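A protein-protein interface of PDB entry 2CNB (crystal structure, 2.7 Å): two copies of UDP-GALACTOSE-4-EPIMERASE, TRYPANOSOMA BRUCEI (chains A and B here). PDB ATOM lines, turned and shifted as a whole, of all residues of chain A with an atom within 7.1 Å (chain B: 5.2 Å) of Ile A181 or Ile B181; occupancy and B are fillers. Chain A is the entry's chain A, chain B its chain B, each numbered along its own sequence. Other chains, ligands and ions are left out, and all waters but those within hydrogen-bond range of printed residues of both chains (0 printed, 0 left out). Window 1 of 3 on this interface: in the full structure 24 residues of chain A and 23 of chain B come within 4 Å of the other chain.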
ATOM      1  N   TYR A 117       5.010 -15.639   6.787  1.00  0.00           N
ATOM      2  CA  TYR A 117       6.418 -15.976   6.823  1.00  0.00           C
ATOM      3  C   TYR A 117       7.307 -14.732   6.801  1.00  0.00           C
ATOM      4  O   TYR A 117       8.277 -14.656   7.555  1.00  0.00           O
ATOM      5  CB  TYR A 117       6.768 -16.927   5.694  1.00  0.00           C
ATOM      6  CG  TYR A 117       6.257 -18.312   5.949  1.00  0.00           C
ATOM      7  CD1 TYR A 117       6.763 -19.067   7.000  1.00  0.00           C
ATOM      8  CD2 TYR A 117       5.268 -18.876   5.137  1.00  0.00           C
ATOM      9  CE1 TYR A 117       6.302 -20.338   7.252  1.00  0.00           C
ATOM     10  CE2 TYR A 117       4.787 -20.165   5.372  1.00  0.00           C
ATOM     11  CZ  TYR A 117       5.309 -20.891   6.437  1.00  0.00           C
ATOM     12  OH  TYR A 117       4.870 -22.168   6.702  1.00  0.00           O
ATOM     13  N   VAL A 121       8.539 -14.293  10.638  1.00  0.00           N
ATOM     14  CA  VAL A 121       9.885 -14.847  10.690  1.00  0.00           C
ATOM     15  C   VAL A 121      10.967 -13.773  10.515  1.00  0.00           C
ATOM     16  O   VAL A 121      11.896 -13.695  11.325  1.00  0.00           O
ATOM     17  CB  VAL A 121      10.095 -15.979   9.690  1.00  0.00           C
ATOM     18  CG1 VAL A 121      11.488 -16.574   9.883  1.00  0.00           C
ATOM     19  CG2 VAL A 121       9.009 -17.041   9.846  1.00  0.00           C
ATOM     20  N   ILE A 124      11.413 -11.510  13.703  1.00  0.00           N
ATOM     21  CA  ILE A 124      12.191 -12.115  14.770  1.00  0.00           C
ATOM     22  C   ILE A 124      13.692 -12.161  14.424  1.00  0.00           C
ATOM     23  O   ILE A 124      14.553 -11.844  15.280  1.00  0.00           O
ATOM     24  CB  ILE A 124      11.642 -13.506  15.161  1.00  0.00           C
ATOM     25  CG1 ILE A 124      12.403 -14.094  16.351  1.00  0.00           C
ATOM     26  CG2 ILE A 124      11.733 -14.458  14.010  1.00  0.00           C
ATOM     27  CD1 ILE A 124      12.459 -13.213  17.567  1.00  0.00           C
ATOM     28  N   PHE A 141       9.571 -14.087  23.996  1.00  0.00           N
ATOM     29  CA  PHE A 141       8.854 -14.102  22.720  1.00  0.00           C
ATOM     30  C   PHE A 141       7.431 -14.604  22.889  1.00  0.00           C
ATOM     31  O   PHE A 141       7.194 -15.596  23.591  1.00  0.00           O
ATOM     32  CB  PHE A 141       9.615 -14.988  21.742  1.00  0.00           C
ATOM     33  CG  PHE A 141       8.864 -15.326  20.483  1.00  0.00           C
ATOM     34  CD1 PHE A 141       8.902 -14.471  19.385  1.00  0.00           C
ATOM     35  CD2 PHE A 141       8.174 -16.539  20.373  1.00  0.00           C
ATOM     36  CE1 PHE A 141       8.244 -14.792  18.228  1.00  0.00           C
ATOM     37  CE2 PHE A 141       7.506 -16.865  19.202  1.00  0.00           C
ATOM     38  CZ  PHE A 141       7.540 -15.990  18.131  1.00  0.00           C
ATOM     39  N   ILE A 147       1.232 -23.727  17.649  1.00  0.00           N
ATOM     40  CA  ILE A 147       2.348 -24.610  17.353  1.00  0.00           C
ATOM     41  C   ILE A 147       1.970 -26.090  17.471  1.00  0.00           C
ATOM     42  O   ILE A 147       2.515 -26.930  16.778  1.00  0.00           O
ATOM     43  CB  ILE A 147       3.607 -24.292  18.206  1.00  0.00           C
ATOM     44  CG1 ILE A 147       3.342 -24.499  19.697  1.00  0.00           C
ATOM     45  CG2 ILE A 147       4.082 -22.881  17.958  1.00  0.00           C
ATOM     46  CD1 ILE A 147       4.616 -24.512  20.532  1.00  0.00           C
ATOM     47  N   PRO A 171       2.018 -27.831  13.447  1.00  0.00           N
ATOM     48  CA  PRO A 171       1.177 -26.684  13.123  1.00  0.00           C
ATOM     49  C   PRO A 171       0.232 -27.001  11.971  1.00  0.00           C
ATOM     50  O   PRO A 171       0.634 -27.695  11.028  1.00  0.00           O
ATOM     51  CB  PRO A 171       2.189 -25.629  12.675  1.00  0.00           C
ATOM     52  CG  PRO A 171       3.408 -25.986  13.383  1.00  0.00           C
ATOM     53  CD  PRO A 171       3.441 -27.479  13.411  1.00  0.00           C
ATOM     54  N   PRO A 174       0.128 -21.713   8.519  1.00  0.00           N
ATOM     55  CA  PRO A 174       1.386 -20.971   8.396  1.00  0.00           C
ATOM     56  C   PRO A 174       1.670 -19.970   9.548  1.00  0.00           C
ATOM     57  O   PRO A 174       2.837 -19.625   9.778  1.00  0.00           O
ATOM     58  CB  PRO A 174       1.246 -20.249   7.050  1.00  0.00           C
ATOM     59  CG  PRO A 174       0.222 -21.012   6.322  1.00  0.00           C
ATOM     60  CD  PRO A 174      -0.744 -21.479   7.365  1.00  0.00           C
ATOM     61  N   GLY A 176       1.016 -20.812  12.721  1.00  0.00           N
ATOM     62  CA  GLY A 176       1.592 -21.730  13.698  1.00  0.00           C
ATOM     63  C   GLY A 176       3.037 -22.059  13.355  1.00  0.00           C
ATOM     64  O   GLY A 176       3.907 -22.087  14.248  1.00  0.00           O
ATOM     65  N   GLU A 177       3.281 -22.295  12.058  1.00  0.00           N
ATOM     66  CA  GLU A 177       4.627 -22.552  11.518  1.00  0.00           C
ATOM     67  C   GLU A 177       5.597 -21.465  11.918  1.00  0.00           C
ATOM     68  O   GLU A 177       6.682 -21.756  12.416  1.00  0.00           O
ATOM     69  CB  GLU A 177       4.616 -22.591   9.985  1.00  0.00           C
ATOM     70  CG  GLU A 177       4.707 -23.962   9.357  1.00  0.00           C
ATOM     71  CD  GLU A 177       5.475 -24.971  10.193  1.00  0.00           C
ATOM     72  OE1 GLU A 177       6.714 -24.830  10.354  1.00  0.00           O
ATOM     73  OE2 GLU A 177       4.813 -25.921  10.672  1.00  0.00           O
ATOM     74  N   SER A 178       5.182 -20.218  11.687  1.00  0.00           N
ATOM     75  CA  SER A 178       6.025 -19.064  11.891  1.00  0.00           C
ATOM     76  C   SER A 178       6.399 -18.863  13.366  1.00  0.00           C
ATOM     77  O   SER A 178       7.497 -18.391  13.669  1.00  0.00           O
ATOM     78  CB  SER A 178       5.385 -17.820  11.270  1.00  0.00           C
ATOM     79  OG  SER A 178       4.259 -17.355  11.989  1.00  0.00           O
ATOM     80  N   LYS A 179       5.515 -19.258  14.283  1.00  0.00           N
ATOM     81  CA  LYS A 179       5.855 -19.254  15.717  1.00  0.00           C
ATOM     82  C   LYS A 179       6.915 -20.296  16.059  1.00  0.00           C
ATOM     83  O   LYS A 179       7.846 -20.022  16.815  1.00  0.00           O
ATOM     84  CB  LYS A 179       4.612 -19.471  16.589  1.00  0.00           C
ATOM     85  CG  LYS A 179       3.653 -18.331  16.559  1.00  0.00           C
ATOM     86  CD  LYS A 179       4.314 -17.104  17.118  1.00  0.00           C
ATOM     87  CE  LYS A 179       3.561 -15.845  16.770  1.00  0.00           C
ATOM     88  NZ  LYS A 179       4.066 -14.702  17.572  1.00  0.00           N
ATOM     89  N   LEU A 180       6.749 -21.495  15.498  1.00  0.00           N
ATOM     90  CA  LEU A 180       7.653 -22.620  15.739  1.00  0.00           C
ATOM     91  C   LEU A 180       9.048 -22.326  15.197  1.00  0.00           C
ATOM     92  O   LEU A 180      10.037 -22.493  15.901  1.00  0.00           O
ATOM     93  CB  LEU A 180       7.081 -23.891  15.111  1.00  0.00           C
ATOM     94  CG  LEU A 180       7.620 -25.237  15.604  1.00  0.00           C
ATOM     95  CD1 LEU A 180       7.729 -25.314  17.143  1.00  0.00           C
ATOM     96  CD2 LEU A 180       6.739 -26.348  15.055  1.00  0.00           C
ATOM     97  N   ILE A 181       9.109 -21.846  13.956  1.00  0.00           N
ATOM     98  CA  ILE A 181      10.361 -21.398  13.341  1.00  0.00           C
ATOM     99  C   ILE A 181      11.103 -20.428  14.256  1.00  0.00           C
ATOM    100  O   ILE A 181      12.305 -20.583  14.485  1.00  0.00           O
ATOM    101  CB  ILE A 181      10.118 -20.787  11.939  1.00  0.00           C
ATOM    102  CG1 ILE A 181       9.784 -21.901  10.944  1.00  0.00           C
ATOM    103  CG2 ILE A 181      11.349 -20.055  11.445  1.00  0.00           C
ATOM    104  CD1 ILE A 181       8.841 -21.523   9.863  1.00  0.00           C
ATOM    105  N   ALA A 182      10.383 -19.442  14.784  1.00  0.00           N
ATOM    106  CA  ALA A 182      10.958 -18.488  15.714  1.00  0.00           C
ATOM    107  C   ALA A 182      11.421 -19.145  17.028  1.00  0.00           C
ATOM    108  O   ALA A 182      12.477 -18.797  17.549  1.00  0.00           O
ATOM    109  CB  ALA A 182       9.982 -17.352  15.979  1.00  0.00           C
ATOM    110  N   GLU A 183      10.667 -20.097  17.572  1.00  0.00           N
ATOM    111  CA  GLU A 183      11.160 -20.801  18.774  1.00  0.00           C
ATOM    112  C   GLU A 183      12.489 -21.501  18.484  1.00  0.00           C
ATOM    113  O   GLU A 183      13.361 -21.570  19.344  1.00  0.00           O
ATOM    114  CB  GLU A 183      10.148 -21.812  19.301  1.00  0.00           C
ATOM    115  CG  GLU A 183       8.884 -21.185  19.821  1.00  0.00           C
ATOM    116  CD  GLU A 183       8.224 -21.986  20.911  1.00  0.00           C
ATOM    117  OE1 GLU A 183       8.803 -23.028  21.306  1.00  0.00           O
ATOM    118  OE2 GLU A 183       7.144 -21.556  21.380  1.00  0.00           O
ATOM    119  N   ARG A 184      12.627 -22.018  17.264  1.00  0.00           N
ATOM    120  CA  ARG A 184      13.840 -22.705  16.827  1.00  0.00           C
ATOM    121  C   ARG A 184      15.005 -21.737  16.714  1.00  0.00           C
ATOM    122  O   ARG A 184      16.073 -21.989  17.258  1.00  0.00           O
ATOM    123  CB  ARG A 184      13.622 -23.401  15.489  1.00  0.00           C
ATOM    124  CG  ARG A 184      12.524 -24.419  15.493  1.00  0.00           C
ATOM    125  CD  ARG A 184      12.833 -25.566  16.424  1.00  0.00           C
ATOM    126  NE  ARG A 184      11.934 -26.691  16.179  1.00  0.00           N
ATOM    127  CZ  ARG A 184      11.158 -27.263  17.096  1.00  0.00           C
ATOM    128  NH1 ARG A 184      11.159 -26.838  18.359  1.00  0.00           N
ATOM    129  NH2 ARG A 184      10.385 -28.287  16.745  1.00  0.00           N
ATOM    130  N   MET A 185      14.799 -20.630  16.014  1.00  0.00           N
ATOM    131  CA  MET A 185      15.837 -19.628  15.895  1.00  0.00           C
ATOM    132  C   MET A 185      16.310 -19.192  17.268  1.00  0.00           C
ATOM    133  O   MET A 185      17.496 -19.164  17.516  1.00  0.00           O
ATOM    134  CB  MET A 185      15.330 -18.425  15.122  1.00  0.00           C
ATOM    135  CG  MET A 185      15.098 -18.695  13.650  1.00  0.00           C
ATOM    136  SD  MET A 185      14.399 -17.241  12.847  1.00  0.00           S
ATOM    137  CE  MET A 185      15.655 -16.030  13.215  1.00  0.00           C
ATOM    138  N   ILE A 186      15.377 -18.881  18.160  1.00  0.00           N
ATOM    139  CA  ILE A 186      15.708 -18.414  19.482  1.00  0.00           C
ATOM    140  C   ILE A 186      16.490 -19.485  20.247  1.00  0.00           C
ATOM    141  O   ILE A 186      17.583 -19.225  20.776  1.00  0.00           O
ATOM    142  CB  ILE A 186      14.444 -17.984  20.213  1.00  0.00           C
ATOM    143  CG1 ILE A 186      13.910 -16.686  19.597  1.00  0.00           C
ATOM    144  CG2 ILE A 186      14.675 -17.866  21.736  1.00  0.00           C
ATOM    145  CD1 ILE A 186      12.421 -16.390  19.918  1.00  0.00           C
ATOM    146  N   ARG A 187      15.949 -20.699  20.263  1.00  0.00           N
ATOM    147  CA  ARG A 187      16.644 -21.852  20.830  1.00  0.00           C
ATOM    148  C   ARG A 187      18.080 -21.970  20.340  1.00  0.00           C
ATOM    149  O   ARG A 187      18.956 -22.283  21.125  1.00  0.00           O
ATOM    150  CB  ARG A 187      15.909 -23.152  20.491  1.00  0.00           C
ATOM    151  CG  ARG A 187      16.597 -24.396  21.078  1.00  0.00           C
ATOM    152  CD  ARG A 187      16.270 -25.655  20.328  1.00  0.00           C
ATOM    153  NE  ARG A 187      16.710 -25.561  18.943  1.00  0.00           N
ATOM    154  CZ  ARG A 187      16.259 -26.340  17.956  1.00  0.00           C
ATOM    155  NH1 ARG A 187      15.341 -27.264  18.203  1.00  0.00           N
ATOM    156  NH2 ARG A 187      16.714 -26.176  16.708  1.00  0.00           N
ATOM    157  N   ASP A 188      18.304 -21.753  19.042  1.00  0.00           N
ATOM    158  CA  ASP A 188      19.613 -21.995  18.427  1.00  0.00           C
ATOM    159  C   ASP A 188      20.593 -20.898  18.766  1.00  0.00           C
ATOM    160  O   ASP A 188      21.803 -21.101  18.745  1.00  0.00           O
ATOM    161  CB  ASP A 188      19.503 -22.228  16.921  1.00  0.00           C
ATOM    162  CG  ASP A 188      18.901 -23.596  16.590  1.00  0.00           C
ATOM    163  OD1 ASP A 188      18.864 -24.466  17.500  1.00  0.00           O
ATOM    164  OD2 ASP A 188      18.440 -23.803  15.440  1.00  0.00           O
ATOM    165  N   VAL B 121      16.837 -18.968   4.720  1.00  0.00           N
ATOM    166  CA  VAL B 121      15.399 -18.701   4.843  1.00  0.00           C
ATOM    167  C   VAL B 121      14.957 -17.407   4.147  1.00  0.00           C
ATOM    168  O   VAL B 121      13.987 -17.421   3.377  1.00  0.00           O
ATOM    169  CB  VAL B 121      14.914 -18.728   6.307  1.00  0.00           C
ATOM    170  CG1 VAL B 121      13.418 -18.443   6.388  1.00  0.00           C
ATOM    171  CG2 VAL B 121      15.213 -20.068   6.919  1.00  0.00           C
ATOM    172  N   GLU B 177      17.597 -27.290   9.841  1.00  0.00           N
ATOM    173  CA  GLU B 177      16.343 -26.586  10.135  1.00  0.00           C
ATOM    174  C   GLU B 177      15.921 -25.680   8.993  1.00  0.00           C
ATOM    175  O   GLU B 177      14.763 -25.687   8.597  1.00  0.00           O
ATOM    176  CB  GLU B 177      16.422 -25.776  11.436  1.00  0.00           C
ATOM    177  CG  GLU B 177      16.165 -26.596  12.698  1.00  0.00           C
ATOM    178  CD  GLU B 177      14.702 -26.902  12.889  1.00  0.00           C
ATOM    179  OE1 GLU B 177      13.913 -26.395  12.072  1.00  0.00           O
ATOM    180  OE2 GLU B 177      14.330 -27.629  13.845  1.00  0.00           O
ATOM    181  N   SER B 178      16.867 -24.907   8.465  1.00  0.00           N
ATOM    182  CA  SER B 178      16.562 -23.921   7.421  1.00  0.00           C
ATOM    183  C   SER B 178      16.086 -24.577   6.126  1.00  0.00           C
ATOM    184  O   SER B 178      15.205 -24.059   5.471  1.00  0.00           O
ATOM    185  CB  SER B 178      17.754 -23.006   7.169  1.00  0.00           C
ATOM    186  OG  SER B 178      18.788 -23.693   6.504  1.00  0.00           O
ATOM    187  N   LYS B 179      16.655 -25.725   5.774  1.00  0.00           N
ATOM    188  CA  LYS B 179      16.181 -26.466   4.606  1.00  0.00           C
ATOM    189  C   LYS B 179      14.762 -26.948   4.884  1.00  0.00           C
ATOM    190  O   LYS B 179      13.890 -26.838   4.040  1.00  0.00           O
ATOM    191  CB  LYS B 179      17.115 -27.638   4.246  1.00  0.00           C
ATOM    192  CG  LYS B 179      18.510 -27.230   3.756  1.00  0.00           C
ATOM    193  CD  LYS B 179      18.454 -26.103   2.704  1.00  0.00           C
ATOM    194  CE  LYS B 179      19.732 -26.017   1.849  1.00  0.00           C
ATOM    195  NZ  LYS B 179      19.497 -25.517   0.449  1.00  0.00           N
ATOM    196  N   LEU B 180      14.533 -27.432   6.096  1.00  0.00           N
ATOM    197  CA  LEU B 180      13.222 -27.897   6.510  1.00  0.00           C
ATOM    198  C   LEU B 180      12.149 -26.817   6.447  1.00  0.00           C
ATOM    199  O   LEU B 180      11.060 -27.059   5.926  1.00  0.00           O
ATOM    200  CB  LEU B 180      13.274 -28.497   7.920  1.00  0.00           C
ATOM    201  CG  LEU B 180      12.012 -29.251   8.337  1.00  0.00           C
ATOM    202  CD1 LEU B 180      11.710 -30.369   7.363  1.00  0.00           C
ATOM    203  CD2 LEU B 180      12.117 -29.792   9.731  1.00  0.00           C
ATOM    204  N   ILE B 181      12.435 -25.629   6.975  1.00  0.00           N
ATOM    205  CA  ILE B 181      11.404 -24.592   7.034  1.00  0.00           C
ATOM    206  C   ILE B 181      11.050 -24.083   5.631  1.00  0.00           C
ATOM    207  O   ILE B 181       9.901 -23.733   5.369  1.00  0.00           O
ATOM    208  CB  ILE B 181      11.716 -23.440   8.068  1.00  0.00           C
ATOM    209  CG1 ILE B 181      12.395 -22.246   7.411  1.00  0.00           C
ATOM    210  CG2 ILE B 181      12.508 -23.926   9.307  1.00  0.00           C
ATOM    211  CD1 ILE B 181      11.500 -21.051   7.320  1.00  0.00           C
ATOM    212  N   ALA B 182      12.031 -24.077   4.729  1.00  0.00           N
ATOM    213  CA  ALA B 182      11.795 -23.717   3.323  1.00  0.00           C
ATOM    214  C   ALA B 182      10.833 -24.714   2.650  1.00  0.00           C
ATOM    215  O   ALA B 182      10.022 -24.344   1.809  1.00  0.00           O
ATOM    216  CB  ALA B 182      13.105 -23.641   2.566  1.00  0.00           C
ATOM    217  N   GLU B 183      10.913 -25.975   3.060  1.00  0.00           N
ATOM    218  CA  GLU B 183      10.019 -26.988   2.544  1.00  0.00           C
ATOM    219  C   GLU B 183       8.585 -26.738   2.969  1.00  0.00           C
ATOM    220  O   GLU B 183       7.676 -26.906   2.156  1.00  0.00           O
ATOM    221  CB  GLU B 183      10.465 -28.393   2.942  1.00  0.00           C
ATOM    222  CG  GLU B 183      11.593 -28.914   2.071  1.00  0.00           C
ATOM    223  CD  GLU B 183      11.739 -30.431   2.098  1.00  0.00           C
ATOM    224  OE1 GLU B 183      10.856 -31.152   2.622  1.00  0.00           O
ATOM    225  OE2 GLU B 183      12.759 -30.906   1.577  1.00  0.00           O
ATOM    226  N   ARG B 184       8.375 -26.333   4.222  1.00  0.00           N
ATOM    227  CA  ARG B 184       7.024 -25.970   4.655  1.00  0.00           C
ATOM    228  C   ARG B 184       6.593 -24.702   3.919  1.00  0.00           C
ATOM    229  O   ARG B 184       5.456 -24.616   3.450  1.00  0.00           O
ATOM    230  CB  ARG B 184       6.914 -25.785   6.170  1.00  0.00           C
ATOM    231  CG  ARG B 184       7.715 -26.765   7.021  1.00  0.00           C
ATOM    232  CD  ARG B 184       7.009 -28.109   7.323  1.00  0.00           C
ATOM    233  NE  ARG B 184       7.846 -28.885   8.251  1.00  0.00           N
ATOM    234  CZ  ARG B 184       7.701 -28.940   9.580  1.00  0.00           C
ATOM    235  NH1 ARG B 184       6.705 -28.313  10.208  1.00  0.00           N
ATOM    236  NH2 ARG B 184       8.549 -29.652  10.297  1.00  0.00           N
ATOM    237  N   MET B 185       7.502 -23.736   3.774  1.00  0.00           N
ATOM    238  CA  MET B 185       7.167 -22.500   3.050  1.00  0.00           C
ATOM    239  C   MET B 185       6.695 -22.788   1.649  1.00  0.00           C
ATOM    240  O   MET B 185       5.726 -22.190   1.188  1.00  0.00           O
ATOM    241  CB  MET B 185       8.342 -21.534   2.982  1.00  0.00           C
ATOM    242  CG  MET B 185       8.371 -20.549   4.122  1.00  0.00           C
ATOM    243  SD  MET B 185       9.931 -19.670   4.269  1.00  0.00           S
ATOM    244  CE  MET B 185       9.793 -18.564   2.877  1.00  0.00           C
ATOM    245  N   ILE B 186       7.399 -23.694   0.980  1.00  0.00           N
ATOM    246  CA  ILE B 186       7.110 -24.030  -0.405  1.00  0.00           C
ATOM    247  C   ILE B 186       5.820 -24.871  -0.500  1.00  0.00           C
ATOM    248  O   ILE B 186       4.979 -24.590  -1.353  1.00  0.00           O
ATOM    249  CB  ILE B 186       8.347 -24.663  -1.102  1.00  0.00           C
ATOM    250  CG1 ILE B 186       9.420 -23.593  -1.351  1.00  0.00           C
ATOM    251  CG2 ILE B 186       7.973 -25.321  -2.409  1.00  0.00           C
ATOM    252  CD1 ILE B 186      10.783 -24.137  -1.734  1.00  0.00           C
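The guanidinium group (NH2) of Arg A187 lies within salt-bridge range of the side-chain carboxylate (OE2) of Glu B177 (3.999 Å). OE2 of Glu A177 is in salt-bridge range of NH1 of Arg B184 (3.1 Å). NE of Arg A184 is in salt-bridge range of OE2 of Glu B177 (3.5 Å).
Ile A181 touches just one residue of chain B: Ile B181. Of chain A, only Ile A181 comes within 4 Å of Ile B181. Printed residues of chain B within 4 Å of Glu A177: Arg B184 (3.1 Å). Of the printed residues of chain B, Tyr A117 touches Met B185. Of the printed residues of chain A, Met B185 touches Tyr A117 (3.6 Å). The nearest printed residue of chain A that does not touch Ile B181 is Tyr A117 (5.1 Å).
The side-chain carboxylate (OD1) of Asp A188 lies within salt-bridge range of the guanidinium group (NE) of Arg A187 (2.8 Å).
Tyr A117 touches Met B185 (CG to CG, 3.6 Å). Ile B181 touches Ile A181 (CD1 to CD1, 3.7 Å).
Printed residues of chain B that touch a printed residue of chain A: Glu B177, Ile B181, Arg B184 and Met B185. Of the 20 printed residues of chain A, 5 touch a printed residue of chain B. Hydrophobic or aromatic side chains of chain A within 4 Å of the printed part of chain B: Tyr A117 and Ile A181. Among the printed residues, 5 pairs touch across the chains.
Glu A177 touches Arg B184, and with the chains exchanged Arg A184 touches Glu B177. Ile B181 touches its own counterpart, Ile A181. Of the 5 pairs that touch across the chains among the printed residues, 3 have their exchanged pair printed and touching as well.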
